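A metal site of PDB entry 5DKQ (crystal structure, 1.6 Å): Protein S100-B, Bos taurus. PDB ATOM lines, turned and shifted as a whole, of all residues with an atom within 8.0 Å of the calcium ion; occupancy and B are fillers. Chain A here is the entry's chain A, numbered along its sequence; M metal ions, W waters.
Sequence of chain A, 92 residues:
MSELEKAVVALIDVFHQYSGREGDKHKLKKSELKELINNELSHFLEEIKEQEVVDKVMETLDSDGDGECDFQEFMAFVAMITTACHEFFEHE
The calcium ion is bound by the backbone carbonyl oxygen (O) of Asp 24, at 2.2 Å.
Water W1 is bound to the calcium ion, at 2.3 Å.
O of Ser 19 binds the calcium ion (2.4 Å).
O of Lys 27 is bound to the calcium ion (2.4 Å).
The calcium ion is bound by O of Glu 22.
The calcium ion is bound by OE1 of Glu 32.
The side-chain carboxylate (OE2) of Glu 32 binds the calcium ion, 2.6 Å away.
The calcium ion has seven donor atoms within binding distance.
OD2 of Asp 24 is in salt-bridge range of NZ of Lys 27 (2.8 Å).
N of His 26 lies within hydrogen-bond range of OD1 of Asp 24, at 3.0 Å.
OG of Ser 19 is in hydrogen-bond range of O of Lys 25 (2.9 Å).
The side-chain hydroxyl (OG) of Ser 19 lies close to the backbone carbonyl oxygen (O) of Phe 15 (3.2 Å).
ND1 of His 16 sits close to OG of Ser 19 (3.5 Å).
OE1 of Glu 22 lies within salt-bridge range of NZ of Lys 29 (3.3 Å).
OE2 of Glu 22 sits at hydrogen-bond distance from OG of Ser 31 (2.6 Å).
OE2 of Glu 32 lies close to N of Arg 21, 3.4 Å away.
Along chain A the residues within 4 Å of the calcium ion span positions 19 to 32.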
ATOM      1  N   PHE A  15     -34.762   7.707 -17.241  1.00  0.00           N
ATOM      2  CA  PHE A  15     -33.695   6.712 -17.279  1.00  0.00           C
ATOM      3  C   PHE A  15     -32.332   7.389 -17.241  1.00  0.00           C
ATOM      4  O   PHE A  15     -31.464   7.046 -16.421  1.00  0.00           O
ATOM      5  CB  PHE A  15     -33.782   5.820 -18.520  1.00  0.00           C
ATOM      6  CG  PHE A  15     -32.677   4.796 -18.594  1.00  0.00           C
ATOM      7  CD1 PHE A  15     -32.749   3.618 -17.844  1.00  0.00           C
ATOM      8  CD2 PHE A  15     -31.564   5.009 -19.391  1.00  0.00           C
ATOM      9  CE1 PHE A  15     -31.720   2.695 -17.884  1.00  0.00           C
ATOM     10  CE2 PHE A  15     -30.533   4.066 -19.441  1.00  0.00           C
ATOM     11  CZ  PHE A  15     -30.627   2.913 -18.695  1.00  0.00           C
ATOM     12  N   HIS A  16     -32.148   8.359 -18.126  1.00  0.00           N
ATOM     13  CA  HIS A  16     -30.841   9.005 -18.251  1.00  0.00           C
ATOM     14  C   HIS A  16     -30.550   9.979 -17.131  1.00  0.00           C
ATOM     15  O   HIS A  16     -29.399  10.285 -16.855  1.00  0.00           O
ATOM     16  CB  HIS A  16     -30.661   9.631 -19.637  1.00  0.00           C
ATOM     17  CG  HIS A  16     -30.358   8.609 -20.689  1.00  0.00           C
ATOM     18  ND1 HIS A  16     -29.129   8.010 -20.806  1.00  0.00           N
ATOM     19  CD2 HIS A  16     -31.137   8.075 -21.662  1.00  0.00           C
ATOM     20  CE1 HIS A  16     -29.154   7.144 -21.800  1.00  0.00           C
ATOM     21  NE2 HIS A  16     -30.356   7.165 -22.336  1.00  0.00           N
ATOM     22  N   TYR A  18     -30.957   9.223 -14.125  1.00  0.00           N
ATOM     23  CA  TYR A  18     -30.373   8.417 -13.067  1.00  0.00           C
ATOM     24  C   TYR A  18     -29.185   7.586 -13.536  1.00  0.00           C
ATOM     25  O   TYR A  18     -28.220   7.423 -12.795  1.00  0.00           O
ATOM     26  CB  TYR A  18     -31.440   7.565 -12.367  1.00  0.00           C
ATOM     27  CG  TYR A  18     -32.314   8.433 -11.506  1.00  0.00           C
ATOM     28  CD1 TYR A  18     -33.416   9.086 -12.033  1.00  0.00           C
ATOM     29  CD2 TYR A  18     -32.000   8.651 -10.177  1.00  0.00           C
ATOM     30  CE1 TYR A  18     -34.192   9.914 -11.262  1.00  0.00           C
ATOM     31  CE2 TYR A  18     -32.773   9.468  -9.384  1.00  0.00           C
ATOM     32  CZ  TYR A  18     -33.864  10.104  -9.925  1.00  0.00           C
ATOM     33  OH  TYR A  18     -34.631  10.935  -9.158  1.00  0.00           O
ATOM     34  N   SER A  19     -29.239   7.103 -14.776  1.00  0.00           N
ATOM     35  CA  SER A  19     -28.198   6.214 -15.301  1.00  0.00           C
ATOM     36  C   SER A  19     -26.840   6.904 -15.434  1.00  0.00           C
ATOM     37  O   SER A  19     -25.793   6.268 -15.352  1.00  0.00           O
ATOM     38  CB  SER A  19     -28.605   5.610 -16.641  1.00  0.00           C
ATOM     39  OG  SER A  19     -28.551   6.574 -17.682  1.00  0.00           O
ATOM     40  N   GLY A  20     -26.858   8.217 -15.645  1.00  0.00           N
ATOM     41  CA  GLY A  20     -25.637   8.960 -15.905  1.00  0.00           C
ATOM     42  C   GLY A  20     -24.900   9.475 -14.669  1.00  0.00           C
ATOM     43  O   GLY A  20     -23.888  10.176 -14.789  1.00  0.00           O
ATOM     44  N   ARG A  21     -25.406   9.140 -13.488  1.00  0.00           N
ATOM     45  CA  ARG A  21     -24.819   9.669 -12.264  1.00  0.00           C
ATOM     46  C   ARG A  21     -23.492   9.007 -11.904  1.00  0.00           C
ATOM     47  O   ARG A  21     -22.567   9.672 -11.430  1.00  0.00           O
ATOM     48  CB  ARG A  21     -25.799   9.529 -11.087  1.00  0.00           C
ATOM     49  CG  ARG A  21     -27.086  10.267 -11.307  1.00  0.00           C
ATOM     50  CD  ARG A  21     -27.962  10.311 -10.095  1.00  0.00           C
ATOM     51  NE  ARG A  21     -29.085  11.224 -10.308  1.00  0.00           N
ATOM     52  CZ  ARG A  21     -29.935  11.601  -9.362  1.00  0.00           C
ATOM     53  NH1 ARG A  21     -29.824  11.143  -8.120  1.00  0.00           N
ATOM     54  NH2 ARG A  21     -30.920  12.438  -9.655  1.00  0.00           N
ATOM     55  N   GLU A  22     -23.412   7.705 -12.140  1.00  0.00           N
ATOM     56  CA  GLU A  22     -22.273   6.878 -11.710  1.00  0.00           C
ATOM     57  C   GLU A  22     -21.880   5.881 -12.773  1.00  0.00           C
ATOM     58  O   GLU A  22     -22.746   5.388 -13.512  1.00  0.00           O
ATOM     59  CB  GLU A  22     -22.632   6.060 -10.473  1.00  0.00           C
ATOM     60  CG  GLU A  22     -23.141   6.827  -9.284  1.00  0.00           C
ATOM     61  CD  GLU A  22     -23.513   5.885  -8.164  1.00  0.00           C
ATOM     62  OE1 GLU A  22     -22.606   5.330  -7.513  1.00  0.00           O
ATOM     63  OE2 GLU A  22     -24.731   5.684  -7.944  1.00  0.00           O
ATOM     64  N   GLY A  23     -20.600   5.526 -12.802  1.00  0.00           N
ATOM     65  CA  GLY A  23     -20.103   4.443 -13.636  1.00  0.00           C
ATOM     66  C   GLY A  23     -20.569   4.479 -15.077  1.00  0.00           C
ATOM     67  O   GLY A  23     -20.479   5.514 -15.747  1.00  0.00           O
ATOM     68  N   ASP A  24     -21.061   3.334 -15.547  1.00  0.00           N
ATOM     69  CA  ASP A  24     -21.619   3.215 -16.878  1.00  0.00           C
ATOM     70  C   ASP A  24     -22.747   4.237 -16.998  1.00  0.00           C
ATOM     71  O   ASP A  24     -23.711   4.186 -16.235  1.00  0.00           O
ATOM     72  CB  ASP A  24     -22.166   1.805 -17.095  1.00  0.00           C
ATOM     73  CG  ASP A  24     -22.412   1.486 -18.549  1.00  0.00           C
ATOM     74  OD1 ASP A  24     -22.815   2.384 -19.306  1.00  0.00           O
ATOM     75  OD2 ASP A  24     -22.189   0.323 -18.945  1.00  0.00           O
ATOM     76  N   LYS A  25     -22.608   5.167 -17.933  1.00  0.00           N
ATOM     77  CA  LYS A  25     -23.590   6.228 -18.060  1.00  0.00           C
ATOM     78  C   LYS A  25     -24.877   5.741 -18.702  1.00  0.00           C
ATOM     79  O   LYS A  25     -25.865   6.464 -18.722  1.00  0.00           O
ATOM     80  CB  LYS A  25     -23.013   7.388 -18.885  1.00  0.00           C
ATOM     81  CG  LYS A  25     -21.824   8.070 -18.234  1.00  0.00           C
ATOM     82  CD  LYS A  25     -21.526   9.398 -18.914  1.00  0.00           C
ATOM     83  CE  LYS A  25     -21.210  10.459 -17.873  1.00  0.00           C
ATOM     84  NZ  LYS A  25     -22.387  10.788 -17.014  1.00  0.00           N
ATOM     85  N   HIS A  26     -24.861   4.521 -19.211  1.00  0.00           N
ATOM     86  CA  HIS A  26     -25.983   4.005 -19.991  1.00  0.00           C
ATOM     87  C   HIS A  26     -26.721   2.905 -19.242  1.00  0.00           C
ATOM     88  O   HIS A  26     -27.619   2.259 -19.790  1.00  0.00           O
ATOM     89  CB  HIS A  26     -25.496   3.496 -21.332  1.00  0.00           C
ATOM     90  CG  HIS A  26     -24.781   4.531 -22.127  1.00  0.00           C
ATOM     91  ND1 HIS A  26     -25.420   5.644 -22.641  1.00  0.00           N
ATOM     92  CD2 HIS A  26     -23.479   4.654 -22.494  1.00  0.00           C
ATOM     93  CE1 HIS A  26     -24.537   6.394 -23.288  1.00  0.00           C
ATOM     94  NE2 HIS A  26     -23.362   5.815 -23.211  1.00  0.00           N
ATOM     95  N   LYS A  27     -26.327   2.676 -17.995  1.00  0.00           N
ATOM     96  CA  LYS A  27     -26.930   1.645 -17.183  1.00  0.00           C
ATOM     97  C   LYS A  27     -27.196   2.148 -15.769  1.00  0.00           C
ATOM     98  O   LYS A  27     -26.477   3.027 -15.257  1.00  0.00           O
ATOM     99  CB  LYS A  27     -26.047   0.380 -17.142  1.00  0.00           C
ATOM    100  CG  LYS A  27     -25.765  -0.272 -18.483  1.00  0.00           C
ATOM    101  CD  LYS A  27     -24.918  -1.524 -18.314  1.00  0.00           C
ATOM    102  CE  LYS A  27     -24.561  -2.143 -19.643  1.00  0.00           C
ATOM    103  NZ  LYS A  27     -23.870  -1.192 -20.549  1.00  0.00           N
ATOM    104  N   LEU A  28     -28.249   1.617 -15.149  1.00  0.00           N
ATOM    105  CA  LEU A  28     -28.501   1.890 -13.752  1.00  0.00           C
ATOM    106  C   LEU A  28     -27.810   0.814 -12.908  1.00  0.00           C
ATOM    107  O   LEU A  28     -28.158  -0.368 -12.984  1.00  0.00           O
ATOM    108  CB  LEU A  28     -30.002   1.851 -13.450  1.00  0.00           C
ATOM    109  CG  LEU A  28     -30.909   2.829 -14.185  1.00  0.00           C
ATOM    110  CD1 LEU A  28     -32.339   2.279 -14.200  1.00  0.00           C
ATOM    111  CD2 LEU A  28     -30.884   4.201 -13.508  1.00  0.00           C
ATOM    112  N   LYS A  29     -26.838   1.211 -12.091  1.00  0.00           N
ATOM    113  CA  LYS A  29     -26.313   0.289 -11.095  1.00  0.00           C
ATOM    114  C   LYS A  29     -27.295   0.336  -9.933  1.00  0.00           C
ATOM    115  O   LYS A  29     -28.197   1.180  -9.927  1.00  0.00           O
ATOM    116  CB  LYS A  29     -24.893   0.669 -10.664  1.00  0.00           C
ATOM    117  CG  LYS A  29     -24.763   2.057 -10.046  1.00  0.00           C
ATOM    118  CD  LYS A  29     -23.281   2.401  -9.876  1.00  0.00           C
ATOM    119  CE  LYS A  29     -22.599   1.484  -8.887  1.00  0.00           C
ATOM    120  NZ  LYS A  29     -22.594   2.064  -7.508  1.00  0.00           N
ATOM    121  N   LYS A  30     -27.152  -0.557  -8.961  1.00  0.00           N
ATOM    122  CA  LYS A  30     -28.142  -0.664  -7.904  1.00  0.00           C
ATOM    123  C   LYS A  30     -28.380   0.647  -7.140  1.00  0.00           C
ATOM    124  O   LYS A  30     -29.496   0.955  -6.753  1.00  0.00           O
ATOM    125  CB  LYS A  30     -27.793  -1.807  -6.926  1.00  0.00           C
ATOM    126  CG  LYS A  30     -28.075  -3.189  -7.469  1.00  0.00           C
ATOM    127  CD  LYS A  30     -27.842  -4.251  -6.407  1.00  0.00           C
ATOM    128  CE  LYS A  30     -26.386  -4.296  -5.989  1.00  0.00           C
ATOM    129  NZ  LYS A  30     -25.518  -4.601  -7.161  1.00  0.00           N
ATOM    130  N   SER A  31     -27.317   1.427  -6.951  1.00  0.00           N
ATOM    131  CA  SER A  31     -27.450   2.683  -6.225  1.00  0.00           C
ATOM    132  C   SER A  31     -28.317   3.689  -6.978  1.00  0.00           C
ATOM    133  O   SER A  31     -29.119   4.410  -6.364  1.00  0.00           O
ATOM    134  CB  SER A  31     -26.075   3.263  -5.866  1.00  0.00           C
ATOM    135  OG  SER A  31     -25.202   3.311  -6.971  1.00  0.00           O
ATOM    136  N   GLU A  32     -28.176   3.708  -8.300  1.00  0.00           N
ATOM    137  CA  GLU A  32     -28.972   4.601  -9.156  1.00  0.00           C
ATOM    138  C   GLU A  32     -30.416   4.143  -9.208  1.00  0.00           C
ATOM    139  O   GLU A  32     -31.337   4.956  -9.092  1.00  0.00           O
ATOM    140  CB  GLU A  32     -28.368   4.638 -10.563  1.00  0.00           C
ATOM    141  CG  GLU A  32     -26.973   5.255 -10.599  1.00  0.00           C
ATOM    142  CD  GLU A  32     -26.276   5.055 -11.911  1.00  0.00           C
ATOM    143  OE1 GLU A  32     -26.501   3.992 -12.540  1.00  0.00           O
ATOM    144  OE2 GLU A  32     -25.499   5.930 -12.326  1.00  0.00           O
ATOM    145  N   LEU A  33     -30.615   2.844  -9.370  1.00  0.00           N
ATOM    146  CA  LEU A  33     -31.950   2.248  -9.363  1.00  0.00           C
ATOM    147  C   LEU A  33     -32.688   2.527  -8.058  1.00  0.00           C
ATOM    148  O   LEU A  33     -33.881   2.822  -8.059  1.00  0.00           O
ATOM    149  CB  LEU A  33     -31.850   0.738  -9.611  1.00  0.00           C
ATOM    150  CG  LEU A  33     -33.165  -0.048  -9.629  1.00  0.00           C
ATOM    151  CD1 LEU A  33     -34.058   0.425 -10.771  1.00  0.00           C
ATOM    152  CD2 LEU A  33     -32.893  -1.542  -9.747  1.00  0.00           C
ATOM    153  N   GLU A  68     -26.505  -4.795 -13.417  1.00  0.00           N
ATOM    154  CA  GLU A  68     -27.016  -3.456 -13.669  1.00  0.00           C
ATOM    155  C   GLU A  68     -28.263  -3.524 -14.533  1.00  0.00           C
ATOM    156  O   GLU A  68     -28.531  -4.537 -15.170  1.00  0.00           O
ATOM    157  CB  GLU A  68     -25.945  -2.611 -14.364  1.00  0.00           C
ATOM    158  CG  GLU A  68     -24.645  -2.455 -13.545  1.00  0.00           C
ATOM    159  CD  GLU A  68     -23.928  -1.143 -13.793  1.00  0.00           C
ATOM    160  OE1 GLU A  68     -24.561  -0.174 -14.277  1.00  0.00           O
ATOM    161  OE2 GLU A  68     -22.712  -1.077 -13.481  1.00  0.00           O
ATOM    162  N   CYS A  69     -29.023  -2.436 -14.563  1.00  0.00           N
ATOM    163  CA  CYS A  69     -30.211  -2.397 -15.397  1.00  0.00           C
ATOM    164  C   CYS A  69     -29.954  -1.498 -16.620  1.00  0.00           C
ATOM    165  O   CYS A  69     -29.802  -0.283 -16.470  1.00  0.00           O
ATOM    166  CB  CYS A  69     -31.373  -1.857 -14.575  1.00  0.00           C
ATOM    167  SG  CYS A  69     -32.946  -1.737 -15.477  1.00  0.00           S
HETATM  168 CA    CA M   1     -24.799   4.403 -14.320  1.00  0.00          CA
HETATM  169  O   HOH W   1     -23.870   2.428 -13.528  1.00  0.00           O
